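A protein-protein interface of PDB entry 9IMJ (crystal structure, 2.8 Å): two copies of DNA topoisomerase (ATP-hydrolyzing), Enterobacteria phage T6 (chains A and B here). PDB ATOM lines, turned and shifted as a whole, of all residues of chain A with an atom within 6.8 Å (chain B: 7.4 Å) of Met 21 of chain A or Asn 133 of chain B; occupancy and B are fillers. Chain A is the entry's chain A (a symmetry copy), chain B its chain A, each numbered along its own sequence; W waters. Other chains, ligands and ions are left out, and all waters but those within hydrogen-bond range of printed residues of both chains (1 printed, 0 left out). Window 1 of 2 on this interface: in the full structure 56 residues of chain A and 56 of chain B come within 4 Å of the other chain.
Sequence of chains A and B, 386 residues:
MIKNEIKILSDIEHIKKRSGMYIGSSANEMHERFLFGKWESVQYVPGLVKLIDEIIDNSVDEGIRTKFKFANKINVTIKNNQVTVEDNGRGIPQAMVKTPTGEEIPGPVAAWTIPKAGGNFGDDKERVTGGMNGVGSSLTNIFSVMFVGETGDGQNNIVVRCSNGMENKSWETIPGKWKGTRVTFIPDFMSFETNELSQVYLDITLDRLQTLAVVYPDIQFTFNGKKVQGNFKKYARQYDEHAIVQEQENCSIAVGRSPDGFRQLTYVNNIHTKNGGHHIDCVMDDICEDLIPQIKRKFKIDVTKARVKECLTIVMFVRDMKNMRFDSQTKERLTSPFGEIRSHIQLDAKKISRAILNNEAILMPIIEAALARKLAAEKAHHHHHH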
ATOM      1  N   LEU A   9      10.948 -27.842 -16.594  1.00  0.00           N
ATOM      2  CA  LEU A   9      11.430 -29.188 -16.324  1.00  0.00           C
ATOM      3  C   LEU A   9      11.395 -29.482 -14.830  1.00  0.00           C
ATOM      4  O   LEU A   9      11.776 -28.647 -14.001  1.00  0.00           O
ATOM      5  CB  LEU A   9      12.872 -29.380 -16.865  1.00  0.00           C
ATOM      6  CG  LEU A   9      13.114 -30.180 -18.161  1.00  0.00           C
ATOM      7  CD1 LEU A   9      12.160 -29.740 -19.252  1.00  0.00           C
ATOM      8  CD2 LEU A   9      14.564 -30.013 -18.639  1.00  0.00           C
ATOM      9  N   HIS A  14      15.264 -32.515 -15.194  1.00  0.00           N
ATOM     10  CA  HIS A  14      16.492 -31.741 -15.348  1.00  0.00           C
ATOM     11  C   HIS A  14      17.718 -32.580 -15.011  1.00  0.00           C
ATOM     12  O   HIS A  14      18.764 -32.462 -15.663  1.00  0.00           O
ATOM     13  CB  HIS A  14      16.439 -30.498 -14.462  1.00  0.00           C
ATOM     14  CG  HIS A  14      17.354 -29.398 -14.906  1.00  0.00           C
ATOM     15  ND1 HIS A  14      18.567 -29.151 -14.301  1.00  0.00           N
ATOM     16  CD2 HIS A  14      17.226 -28.474 -15.889  1.00  0.00           C
ATOM     17  CE1 HIS A  14      19.165 -28.148 -14.920  1.00  0.00           C
ATOM     18  NE2 HIS A  14      18.371 -27.716 -15.885  1.00  0.00           N
ATOM     19  N   LYS A  17      18.118 -34.729 -17.947  1.00  0.00           N
ATOM     20  CA  LYS A  17      18.435 -34.056 -19.203  1.00  0.00           C
ATOM     21  C   LYS A  17      19.790 -33.368 -19.184  1.00  0.00           C
ATOM     22  O   LYS A  17      20.480 -33.333 -20.204  1.00  0.00           O
ATOM     23  CB  LYS A  17      17.364 -33.035 -19.564  1.00  0.00           C
ATOM     24  CG  LYS A  17      17.729 -32.231 -20.821  1.00  0.00           C
ATOM     25  CD  LYS A  17      17.461 -32.947 -22.115  1.00  0.00           C
ATOM     26  CE  LYS A  17      16.934 -31.949 -23.141  1.00  0.00           C
ATOM     27  NZ  LYS A  17      16.160 -32.559 -24.267  1.00  0.00           N
ATOM     28  N   ARG A  18      20.175 -32.778 -18.057  1.00  0.00           N
ATOM     29  CA  ARG A  18      21.474 -32.127 -17.966  1.00  0.00           C
ATOM     30  C   ARG A  18      22.377 -32.891 -17.007  1.00  0.00           C
ATOM     31  O   ARG A  18      23.030 -32.292 -16.146  1.00  0.00           O
ATOM     32  CB  ARG A  18      21.310 -30.676 -17.533  1.00  0.00           C
ATOM     33  CG  ARG A  18      20.537 -29.857 -18.529  1.00  0.00           C
ATOM     34  CD  ARG A  18      21.279 -29.741 -19.874  1.00  0.00           C
ATOM     35  NE  ARG A  18      20.523 -29.006 -20.891  1.00  0.00           N
ATOM     36  CZ  ARG A  18      20.190 -29.508 -22.072  1.00  0.00           C
ATOM     37  NH1 ARG A  18      20.451 -30.766 -22.387  1.00  0.00           N
ATOM     38  NH2 ARG A  18      19.569 -28.732 -22.953  1.00  0.00           N
ATOM     39  N   SER A  19      22.453 -34.219 -17.190  1.00  0.00           N
ATOM     40  CA  SER A  19      23.069 -35.075 -16.176  1.00  0.00           C
ATOM     41  C   SER A  19      24.501 -34.664 -15.848  1.00  0.00           C
ATOM     42  O   SER A  19      24.946 -34.840 -14.709  1.00  0.00           O
ATOM     43  CB  SER A  19      23.044 -36.532 -16.625  1.00  0.00           C
ATOM     44  OG  SER A  19      24.186 -36.840 -17.390  1.00  0.00           O
ATOM     45  N   GLY A  20      25.238 -34.128 -16.816  1.00  0.00           N
ATOM     46  CA  GLY A  20      26.660 -33.912 -16.613  1.00  0.00           C
ATOM     47  C   GLY A  20      27.015 -32.706 -15.781  1.00  0.00           C
ATOM     48  O   GLY A  20      28.156 -32.591 -15.337  1.00  0.00           O
ATOM     49  N   MET A  21      26.073 -31.796 -15.579  1.00  0.00           N
ATOM     50  CA  MET A  21      26.208 -30.741 -14.586  1.00  0.00           C
ATOM     51  C   MET A  21      25.953 -31.268 -13.177  1.00  0.00           C
ATOM     52  O   MET A  21      26.283 -30.591 -12.194  1.00  0.00           O
ATOM     53  CB  MET A  21      25.252 -29.591 -14.988  1.00  0.00           C
ATOM     54  CG  MET A  21      24.616 -28.772 -13.876  1.00  0.00           C
ATOM     55  SD  MET A  21      23.231 -27.771 -14.491  1.00  0.00           S
ATOM     56  CE  MET A  21      22.234 -27.487 -12.992  1.00  0.00           C
ATOM     57  N   TYR A  22      25.407 -32.484 -13.073  1.00  0.00           N
ATOM     58  CA  TYR A  22      25.114 -33.157 -11.812  1.00  0.00           C
ATOM     59  C   TYR A  22      26.095 -34.255 -11.441  1.00  0.00           C
ATOM     60  O   TYR A  22      26.340 -34.447 -10.252  1.00  0.00           O
ATOM     61  CB  TYR A  22      23.720 -33.779 -11.855  1.00  0.00           C
ATOM     62  CG  TYR A  22      22.630 -32.754 -11.845  1.00  0.00           C
ATOM     63  CD1 TYR A  22      22.124 -32.266 -10.654  1.00  0.00           C
ATOM     64  CD2 TYR A  22      22.105 -32.259 -13.034  1.00  0.00           C
ATOM     65  CE1 TYR A  22      21.115 -31.300 -10.656  1.00  0.00           C
ATOM     66  CE2 TYR A  22      21.107 -31.302 -13.039  1.00  0.00           C
ATOM     67  CZ  TYR A  22      20.613 -30.820 -11.853  1.00  0.00           C
ATOM     68  OH  TYR A  22      19.622 -29.857 -11.864  1.00  0.00           O
ATOM     69  N   ILE A  23      26.637 -35.004 -12.413  1.00  0.00           N
ATOM     70  CA  ILE A  23      27.475 -36.154 -12.095  1.00  0.00           C
ATOM     71  C   ILE A  23      28.722 -36.244 -12.981  1.00  0.00           C
ATOM     72  O   ILE A  23      29.699 -36.899 -12.606  1.00  0.00           O
ATOM     73  CB  ILE A  23      26.658 -37.459 -12.178  1.00  0.00           C
ATOM     74  CG1 ILE A  23      25.992 -37.584 -13.533  1.00  0.00           C
ATOM     75  CG2 ILE A  23      25.604 -37.551 -11.083  1.00  0.00           C
ATOM     76  CD1 ILE A  23      26.015 -39.004 -14.034  1.00  0.00           C
ATOM     77  N   GLY A  24      28.721 -35.630 -14.160  1.00  0.00           N
ATOM     78  CA  GLY A  24      29.891 -35.718 -15.029  1.00  0.00           C
ATOM     79  C   GLY A  24      29.693 -36.591 -16.268  1.00  0.00           C
ATOM     80  O   GLY A  24      28.579 -36.994 -16.635  1.00  0.00           O
ATOM     81  N   SER A 328      30.644 -26.723  -8.448  1.00  0.00           N
ATOM     82  CA  SER A 328      29.844 -27.675  -9.195  1.00  0.00           C
ATOM     83  C   SER A 328      29.320 -28.697  -8.218  1.00  0.00           C
ATOM     84  O   SER A 328      29.876 -28.870  -7.137  1.00  0.00           O
ATOM     85  CB  SER A 328      30.658 -28.380 -10.276  1.00  0.00           C
ATOM     86  OG  SER A 328      31.090 -29.633  -9.789  1.00  0.00           O
ATOM     87  N   GLN A 329      28.254 -29.390  -8.613  1.00  0.00           N
ATOM     88  CA  GLN A 329      27.803 -30.497  -7.788  1.00  0.00           C
ATOM     89  C   GLN A 329      28.890 -31.563  -7.611  1.00  0.00           C
ATOM     90  O   GLN A 329      28.871 -32.280  -6.605  1.00  0.00           O
ATOM     91  CB  GLN A 329      26.522 -31.098  -8.381  1.00  0.00           C
ATOM     92  CG  GLN A 329      26.105 -32.519  -7.883  1.00  0.00           C
ATOM     93  CD  GLN A 329      25.786 -32.623  -6.365  1.00  0.00           C
ATOM     94  OE1 GLN A 329      25.523 -31.634  -5.694  1.00  0.00           O
ATOM     95  NE2 GLN A 329      25.809 -33.845  -5.841  1.00  0.00           N
ATOM     96  N   THR A 330      29.864 -31.670  -8.525  1.00  0.00           N
ATOM     97  CA  THR A 330      30.841 -32.763  -8.416  1.00  0.00           C
ATOM     98  C   THR A 330      31.949 -32.490  -7.411  1.00  0.00           C
ATOM     99  O   THR A 330      32.833 -33.336  -7.268  1.00  0.00           O
ATOM    100  CB  THR A 330      31.491 -33.113  -9.769  1.00  0.00           C
ATOM    101  OG1 THR A 330      31.947 -31.927 -10.428  1.00  0.00           O
ATOM    102  CG2 THR A 330      30.519 -33.855 -10.655  1.00  0.00           C
ATOM    103  N   MET B  21      27.639 -23.230  -6.412  1.00  0.00           N
ATOM    104  CA  MET B  21      27.442 -24.286  -7.393  1.00  0.00           C
ATOM    105  C   MET B  21      26.658 -23.783  -8.602  1.00  0.00           C
ATOM    106  O   MET B  21      26.630 -24.453  -9.643  1.00  0.00           O
ATOM    107  CB  MET B  21      26.757 -25.475  -6.675  1.00  0.00           C
ATOM    108  CG  MET B  21      25.792 -26.332  -7.478  1.00  0.00           C
ATOM    109  SD  MET B  21      24.782 -27.389  -6.402  1.00  0.00           S
ATOM    110  CE  MET B  21      23.313 -27.731  -7.425  1.00  0.00           C
ATOM    111  N   TYR B  22      26.057 -22.594  -8.485  1.00  0.00           N
ATOM    112  CA  TYR B  22      25.287 -21.947  -9.541  1.00  0.00           C
ATOM    113  C   TYR B  22      26.009 -20.808 -10.240  1.00  0.00           C
ATOM    114  O   TYR B  22      25.785 -20.616 -11.433  1.00  0.00           O
ATOM    115  CB  TYR B  22      23.982 -21.389  -8.977  1.00  0.00           C
ATOM    116  CG  TYR B  22      23.013 -22.462  -8.590  1.00  0.00           C
ATOM    117  CD1 TYR B  22      22.125 -22.983  -9.513  1.00  0.00           C
ATOM    118  CD2 TYR B  22      22.991 -22.971  -7.296  1.00  0.00           C
ATOM    119  CE1 TYR B  22      21.233 -23.995  -9.144  1.00  0.00           C
ATOM    120  CE2 TYR B  22      22.111 -23.972  -6.929  1.00  0.00           C
ATOM    121  CZ  TYR B  22      21.235 -24.486  -7.851  1.00  0.00           C
ATOM    122  OH  TYR B  22      20.364 -25.493  -7.480  1.00  0.00           O
ATOM    123  N   PRO B 115      13.451 -20.959 -12.579  1.00  0.00           N
ATOM    124  CA  PRO B 115      14.586 -21.839 -12.868  1.00  0.00           C
ATOM    125  C   PRO B 115      14.107 -23.144 -13.472  1.00  0.00           C
ATOM    126  O   PRO B 115      13.060 -23.680 -13.084  1.00  0.00           O
ATOM    127  CB  PRO B 115      15.221 -22.070 -11.490  1.00  0.00           C
ATOM    128  CG  PRO B 115      14.709 -20.986 -10.651  1.00  0.00           C
ATOM    129  CD  PRO B 115      13.325 -20.693 -11.145  1.00  0.00           C
ATOM    130  N   LYS B 116      14.907 -23.668 -14.407  1.00  0.00           N
ATOM    131  CA  LYS B 116      14.522 -24.849 -15.173  1.00  0.00           C
ATOM    132  C   LYS B 116      13.436 -24.490 -16.196  1.00  0.00           C
ATOM    133  O   LYS B 116      12.502 -25.253 -16.436  1.00  0.00           O
ATOM    134  CB  LYS B 116      14.087 -26.003 -14.249  1.00  0.00           C
ATOM    135  CG  LYS B 116      15.232 -26.653 -13.461  1.00  0.00           C
ATOM    136  CD  LYS B 116      14.759 -27.340 -12.200  1.00  0.00           C
ATOM    137  CE  LYS B 116      15.965 -27.866 -11.455  1.00  0.00           C
ATOM    138  NZ  LYS B 116      15.646 -28.319 -10.084  1.00  0.00           N
ATOM    139  N   ALA B 117      13.578 -23.320 -16.821  1.00  0.00           N
ATOM    140  CA  ALA B 117      12.617 -22.841 -17.803  1.00  0.00           C
ATOM    141  C   ALA B 117      13.383 -22.074 -18.860  1.00  0.00           C
ATOM    142  O   ALA B 117      13.915 -20.989 -18.591  1.00  0.00           O
ATOM    143  CB  ALA B 117      11.555 -21.954 -17.162  1.00  0.00           C
ATOM    144  N   GLY B 118      13.423 -22.627 -20.059  1.00  0.00           N
ATOM    145  CA  GLY B 118      14.032 -21.911 -21.156  1.00  0.00           C
ATOM    146  C   GLY B 118      13.729 -22.576 -22.475  1.00  0.00           C
ATOM    147  O   GLY B 118      12.946 -23.528 -22.554  1.00  0.00           O
ATOM    148  N   ASN B 120      16.147 -23.936 -24.590  1.00  0.00           N
ATOM    149  CA  ASN B 120      17.273 -24.770 -24.994  1.00  0.00           C
ATOM    150  C   ASN B 120      17.126 -26.174 -24.427  1.00  0.00           C
ATOM    151  O   ASN B 120      18.100 -26.813 -24.038  1.00  0.00           O
ATOM    152  CB  ASN B 120      18.593 -24.133 -24.571  1.00  0.00           C
ATOM    153  CG  ASN B 120      18.727 -22.694 -25.067  1.00  0.00           C
ATOM    154  OD1 ASN B 120      18.543 -22.423 -26.255  1.00  0.00           O
ATOM    155  ND2 ASN B 120      19.038 -21.767 -24.157  1.00  0.00           N
ATOM    156  N   PHE B 121      15.893 -26.678 -24.378  1.00  0.00           N
ATOM    157  CA  PHE B 121      15.632 -28.030 -23.906  1.00  0.00           C
ATOM    158  C   PHE B 121      15.170 -28.942 -25.032  1.00  0.00           C
ATOM    159  O   PHE B 121      14.337 -29.831 -24.806  1.00  0.00           O
ATOM    160  CB  PHE B 121      14.598 -28.032 -22.790  1.00  0.00           C
ATOM    161  CG  PHE B 121      15.107 -27.503 -21.486  1.00  0.00           C
ATOM    162  CD1 PHE B 121      16.312 -27.934 -20.972  1.00  0.00           C
ATOM    163  CD2 PHE B 121      14.357 -26.604 -20.757  1.00  0.00           C
ATOM    164  CE1 PHE B 121      16.757 -27.463 -19.762  1.00  0.00           C
ATOM    165  CE2 PHE B 121      14.790 -26.133 -19.553  1.00  0.00           C
ATOM    166  CZ  PHE B 121      15.989 -26.557 -19.050  1.00  0.00           C
ATOM    167  N   ARG B 127      21.559 -29.141 -30.524  1.00  0.00           N
ATOM    168  CA  ARG B 127      21.639 -27.887 -29.783  1.00  0.00           C
ATOM    169  C   ARG B 127      22.971 -27.201 -30.053  1.00  0.00           C
ATOM    170  O   ARG B 127      24.037 -27.719 -29.698  1.00  0.00           O
ATOM    171  CB  ARG B 127      21.454 -28.131 -28.289  1.00  0.00           C
ATOM    172  CG  ARG B 127      21.535 -26.857 -27.496  1.00  0.00           C
ATOM    173  CD  ARG B 127      21.547 -27.109 -26.014  1.00  0.00           C
ATOM    174  NE  ARG B 127      22.787 -27.738 -25.588  1.00  0.00           N
ATOM    175  CZ  ARG B 127      22.895 -29.003 -25.203  1.00  0.00           C
ATOM    176  NH1 ARG B 127      21.843 -29.808 -25.158  1.00  0.00           N
ATOM    177  NH2 ARG B 127      24.085 -29.474 -24.855  1.00  0.00           N
ATOM    178  N   GLY B 130      24.976 -21.816 -26.763  1.00  0.00           N
ATOM    179  CA  GLY B 130      25.643 -21.921 -25.478  1.00  0.00           C
ATOM    180  C   GLY B 130      24.696 -22.104 -24.308  1.00  0.00           C
ATOM    181  O   GLY B 130      25.131 -22.499 -23.222  1.00  0.00           O
ATOM    182  N   GLY B 131      23.419 -21.814 -24.484  1.00  0.00           N
ATOM    183  CA  GLY B 131      22.483 -21.921 -23.398  1.00  0.00           C
ATOM    184  C   GLY B 131      21.887 -23.299 -23.448  1.00  0.00           C
ATOM    185  O   GLY B 131      21.732 -23.862 -24.527  1.00  0.00           O
ATOM    186  N   MET B 132      21.583 -23.846 -22.271  1.00  0.00           N
ATOM    187  CA  MET B 132      21.097 -25.214 -22.202  1.00  0.00           C
ATOM    188  C   MET B 132      20.419 -25.548 -20.882  1.00  0.00           C
ATOM    189  O   MET B 132      19.634 -26.500 -20.812  1.00  0.00           O
ATOM    190  CB  MET B 132      22.247 -26.195 -22.419  1.00  0.00           C
ATOM    191  CG  MET B 132      23.143 -26.407 -21.196  1.00  0.00           C
ATOM    192  SD  MET B 132      24.856 -26.786 -21.596  1.00  0.00           S
ATOM    193  CE  MET B 132      24.722 -28.556 -21.785  1.00  0.00           C
ATOM    194  N   ASN B 133      20.742 -24.845 -19.808  1.00  0.00           N
ATOM    195  CA  ASN B 133      20.231 -25.342 -18.546  1.00  0.00           C
ATOM    196  C   ASN B 133      18.922 -24.704 -18.147  1.00  0.00           C
ATOM    197  O   ASN B 133      18.152 -25.333 -17.419  1.00  0.00           O
ATOM    198  CB  ASN B 133      21.254 -25.157 -17.438  1.00  0.00           C
ATOM    199  CG  ASN B 133      22.451 -26.087 -17.585  1.00  0.00           C
ATOM    200  OD1 ASN B 133      22.332 -27.234 -18.034  1.00  0.00           O
ATOM    201  ND2 ASN B 133      23.617 -25.599 -17.182  1.00  0.00           N
ATOM    202  N   GLY B 134      18.646 -23.490 -18.617  1.00  0.00           N
ATOM    203  CA  GLY B 134      17.406 -22.809 -18.289  1.00  0.00           C
ATOM    204  C   GLY B 134      17.402 -22.201 -16.907  1.00  0.00           C
ATOM    205  O   GLY B 134      16.386 -22.289 -16.193  1.00  0.00           O
ATOM    206  N   VAL B 135      18.518 -21.592 -16.492  1.00  0.00           N
ATOM    207  CA  VAL B 135      18.618 -21.090 -15.131  1.00  0.00           C
ATOM    208  C   VAL B 135      19.372 -19.769 -15.046  1.00  0.00           C
ATOM    209  O   VAL B 135      19.157 -18.991 -14.115  1.00  0.00           O
ATOM    210  CB  VAL B 135      19.284 -22.141 -14.228  1.00  0.00           C
ATOM    211  CG1 VAL B 135      18.321 -23.325 -13.940  1.00  0.00           C
ATOM    212  CG2 VAL B 135      20.550 -22.621 -14.892  1.00  0.00           C
ATOM    213  N   GLY B 136      20.254 -19.487 -16.004  1.00  0.00           N
ATOM    214  CA  GLY B 136      21.146 -18.338 -15.858  1.00  0.00           C
ATOM    215  C   GLY B 136      20.454 -16.988 -15.686  1.00  0.00           C
ATOM    216  O   GLY B 136      20.961 -16.113 -14.971  1.00  0.00           O
ATOM    217  N   ARG B 325      28.871 -29.870 -23.527  1.00  0.00           N
ATOM    218  CA  ARG B 325      28.560 -30.395 -22.209  1.00  0.00           C
ATOM    219  C   ARG B 325      29.637 -29.978 -21.237  1.00  0.00           C
ATOM    220  O   ARG B 325      30.819 -29.910 -21.591  1.00  0.00           O
ATOM    221  CB  ARG B 325      28.467 -31.903 -22.223  1.00  0.00           C
ATOM    222  CG  ARG B 325      27.218 -32.418 -22.860  1.00  0.00           C
ATOM    223  CD  ARG B 325      27.536 -33.764 -23.432  1.00  0.00           C
ATOM    224  NE  ARG B 325      27.904 -33.683 -24.835  1.00  0.00           N
ATOM    225  CZ  ARG B 325      27.778 -34.693 -25.681  1.00  0.00           C
ATOM    226  NH1 ARG B 325      27.423 -35.902 -25.264  1.00  0.00           N
ATOM    227  NH2 ARG B 325      28.026 -34.490 -26.971  1.00  0.00           N
ATOM    228  N   PHE B 326      29.225 -29.737 -20.000  1.00  0.00           N
ATOM    229  CA  PHE B 326      30.106 -29.177 -19.002  1.00  0.00           C
ATOM    230  C   PHE B 326      29.798 -29.829 -17.690  1.00  0.00           C
ATOM    231  O   PHE B 326      28.749 -30.449 -17.519  1.00  0.00           O
ATOM    232  CB  PHE B 326      29.913 -27.681 -18.857  1.00  0.00           C
ATOM    233  CG  PHE B 326      29.957 -26.957 -20.143  1.00  0.00           C
ATOM    234  CD1 PHE B 326      31.167 -26.495 -20.645  1.00  0.00           C
ATOM    235  CD2 PHE B 326      28.800 -26.746 -20.861  1.00  0.00           C
ATOM    236  CE1 PHE B 326      31.216 -25.820 -21.845  1.00  0.00           C
ATOM    237  CE2 PHE B 326      28.842 -26.063 -22.062  1.00  0.00           C
ATOM    238  CZ  PHE B 326      30.050 -25.595 -22.553  1.00  0.00           C
ATOM    239  N   ASP B 327      30.697 -29.623 -16.740  1.00  0.00           N
ATOM    240  CA  ASP B 327      30.600 -30.226 -15.421  1.00  0.00           C
ATOM    241  C   ASP B 327      29.999 -29.294 -14.376  1.00  0.00           C
ATOM    242  O   ASP B 327      30.048 -29.605 -13.187  1.00  0.00           O
ATOM    243  CB  ASP B 327      31.977 -30.660 -14.955  1.00  0.00           C
ATOM    244  CG  ASP B 327      32.989 -29.566 -15.103  1.00  0.00           C
ATOM    245  OD1 ASP B 327      32.604 -28.441 -15.529  1.00  0.00           O
ATOM    246  OD2 ASP B 327      34.172 -29.825 -14.805  1.00  0.00           O
ATOM    247  N   SER B 328      29.458 -28.152 -14.776  1.00  0.00           N
ATOM    248  CA  SER B 328      28.951 -27.230 -13.776  1.00  0.00           C
ATOM    249  C   SER B 328      28.055 -26.241 -14.479  1.00  0.00           C
ATOM    250  O   SER B 328      28.160 -26.053 -15.688  1.00  0.00           O
ATOM    251  CB  SER B 328      30.075 -26.480 -13.068  1.00  0.00           C
ATOM    252  OG  SER B 328      30.237 -25.212 -13.671  1.00  0.00           O
ATOM    253  N   GLN B 329      27.182 -25.595 -13.710  1.00  0.00           N
ATOM    254  CA  GLN B 329      26.406 -24.517 -14.299  1.00  0.00           C
ATOM    255  C   GLN B 329      27.299 -23.403 -14.857  1.00  0.00           C
ATOM    256  O   GLN B 329      26.875 -22.697 -15.778  1.00  0.00           O
ATOM    257  CB  GLN B 329      25.411 -23.969 -13.268  1.00  0.00           C
ATOM    258  CG  GLN B 329      24.774 -22.573 -13.562  1.00  0.00           C
ATOM    259  CD  GLN B 329      23.909 -22.497 -14.852  1.00  0.00           C
ATOM    260  OE1 GLN B 329      23.461 -23.503 -15.386  1.00  0.00           O
ATOM    261  NE2 GLN B 329      23.680 -21.280 -15.336  1.00  0.00           N
ATOM    262  N   THR B 330      28.538 -23.244 -14.370  1.00  0.00           N
ATOM    263  CA  THR B 330      29.353 -22.109 -14.825  1.00  0.00           C
ATOM    264  C   THR B 330      30.019 -22.340 -16.172  1.00  0.00           C
ATOM    265  O   THR B 330      30.748 -21.456 -16.626  1.00  0.00           O
ATOM    266  CB  THR B 330      30.443 -21.718 -13.807  1.00  0.00           C
ATOM    267  OG1 THR B 330      31.164 -22.876 -13.376  1.00  0.00           O
ATOM    268  CG2 THR B 330      29.837 -21.013 -12.617  1.00  0.00           C
ATOM    269  N   LYS B 331      29.773 -23.483 -16.810  1.00  0.00           N
ATOM    270  CA  LYS B 331      30.178 -23.753 -18.193  1.00  0.00           C
ATOM    271  C   LYS B 331      31.674 -23.481 -18.418  1.00  0.00           C
ATOM    272  O   LYS B 331      32.097 -23.018 -19.480  1.00  0.00           O
ATOM    273  CB  LYS B 331      29.310 -22.954 -19.183  1.00  0.00           C
ATOM    274  CG  LYS B 331      27.977 -23.607 -19.593  1.00  0.00           C
ATOM    275  CD  LYS B 331      26.900 -22.615 -20.091  1.00  0.00           C
ATOM    276  CE  LYS B 331      25.469 -23.164 -19.862  1.00  0.00           C
ATOM    277  NZ  LYS B 331      24.242 -22.247 -20.149  1.00  0.00           N
ATOM    278  N   THR B 335      33.162 -30.594 -21.395  1.00  0.00           N
ATOM    279  CA  THR B 335      33.263 -31.967 -20.928  1.00  0.00           C
ATOM    280  C   THR B 335      32.707 -32.981 -21.942  1.00  0.00           C
ATOM    281  O   THR B 335      32.506 -34.151 -21.594  1.00  0.00           O
ATOM    282  CB  THR B 335      32.576 -32.054 -19.560  1.00  0.00           C
ATOM    283  OG1 THR B 335      33.142 -33.126 -18.803  1.00  0.00           O
ATOM    284  CG2 THR B 335      31.074 -32.261 -19.700  1.00  0.00           C
HETATM  285  O   HOH W   1      19.140 -28.935 -25.765  1.00  0.00           O
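Hydrophobic or aromatic side chains of chain A within 4 Å of the printed part of chain B: Leu 9, His 14 and Met 21. Printed residues of chain B that touch a printed residue of chain A: Lys 116, Asn 120, Phe 121, Arg 127, Met 132, Asn 133, Phe 326, Asp 327 and Ser 328. Hydrophobic or aromatic side chains of chain B within 4 Å of the printed part of chain A: Phe 121 and Met 132. Among the printed residues, no Asp or Glu carboxylate lies within 4 Å of a Lys or Arg side-chain nitrogen of the other chain.
Ser 328 of chain A touches its own counterpart, Ser 328 of chain B. 5 positions are printed for both chains.
The backbone NH (N) of Lys 116 of chain B lies within hydrogen-bond range of the backbone carbonyl oxygen (O) of Gly 134 of chain B. The side-chain amide nitrogen of Asn 120 of chain B lies close to the backbone carbonyl oxygen of Gly 131 of chain B (3.4 Å). The side-chain amide nitrogen of Asn 133 of chain B lies within hydrogen-bond range of the side-chain amide oxygen of Gln 329 of chain B (2.8 Å). The side-chain hydroxyl (OG1) of Thr 330 of chain B is in hydrogen-bond range of the side-chain hydroxyl (OG) of Ser 328 of chain B, at 2.5 Å. The side-chain hydroxyl of Thr 330 of chain A is in hydrogen-bond range of the side-chain hydroxyl of Ser 328 of chain A (2.5 Å).
Phe 121 of chain B touches Leu 9 of chain A. His 14 of chain A touches Lys 116 of chain B (CD2 to CG, 3.6 Å). Phe 121 of chain B touches His 14 of chain A (CZ to CD2, 3.9 Å). NH2 of Arg 18 of chain A touches CD1 of Phe 121 of chain B, at 3.9 Å. OD1 of Asn 133 of chain B touches CG of Arg 18 of chain A, 3.2 Å away. Asp 327 of chain B touches Gly 20 of chain A. O of Phe 326 of chain B touches N of Met 21 of chain A, 3.6 Å away. CB of Ser 328 of chain A touches O of Asp 327 of chain B, at 3.2 Å. CB of Ser 328 of chain B touches CB of Ser 328 of chain A, at 3.4 Å.
Printed residues of chain B within 4 Å of Met 21 of chain A: Asn 133 and Phe 326. Of chain A, only His 14 (2.8 Å), Arg 18 (3.2 Å) and Met 21 (3.5 Å) come within 4 Å of Asn 133 of chain B. Of chain B, only Phe 326 and Asp 327 come within 4 Å of Gly 20 of chain A. Printed residues of chain A within 4 Å of Lys 116 of chain B: Leu 9 (3.0 Å) and His 14 (3.6 Å). Of the printed residues of chain B, Leu 9 of chain A touches Lys 116 and Phe 121. Printed residues of chain B within 4 Å of Ser 328 of chain A: Asp 327 and Ser 328. Of the printed residues of chain A, Met 132 of chain B touches Arg 18 (2.7 Å). Arg 325 of chain B touches none of the printed residues of chain A. Gly 118 of chain B touches none of the printed residues of chain A. The nearest printed residue of chain B that does not touch Met 21 of chain A is Asp 327 of chain B (4.02 Å). The nearest residue of chain A that does not touch Asn 133 of chain B is Leu 9 of chain A (6.0 Å).
Water W1 lies within hydrogen-bond range of the guanidinium group (NH2) of Arg 18 of chain A (2.9 Å), the guanidinium group (NH1) of Arg 127 of chain B (2.9 Å) and the backbone carbonyl oxygen (O) of Asn 120 of chain B (2.9 Å).
The backbone carbonyl oxygen of Lys 116 of chain B is in hydrogen-bond range of the backbone NH of Leu 9 of chain A, at 3.0 Å. O of Asn 120 of chain B lies within hydrogen-bond range of NH2 of Arg 18 of chain A, 2.6 Å away. The backbone carbonyl oxygen (O) of Phe 121 of chain B sits at hydrogen-bond distance from the side-chain amino group (NZ) of Lys 17 of chain A, at 3.3 Å. The backbone carbonyl oxygen (O) of Met 132 of chain B is in hydrogen-bond range of the guanidinium group (NE) of Arg 18 of chain A (2.7 Å). The backbone carbonyl oxygen of Asn 133 of chain B lies within hydrogen-bond range of a ring nitrogen (NE2) of His 14 of chain A. SD of Met 21 of chain A sits at hydrogen-bond distance from ND2 of Asn 133 of chain B (3.5 Å). The guanidinium group (NH1) of Arg 18 of chain A lies close to the guanidinium group (NH1) of Arg 127 of chain B (3.2 Å). The backbone carbonyl oxygen (O) of Phe 326 of chain B sits close to the backbone carbonyl oxygen (O) of Gly 20 of chain A.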
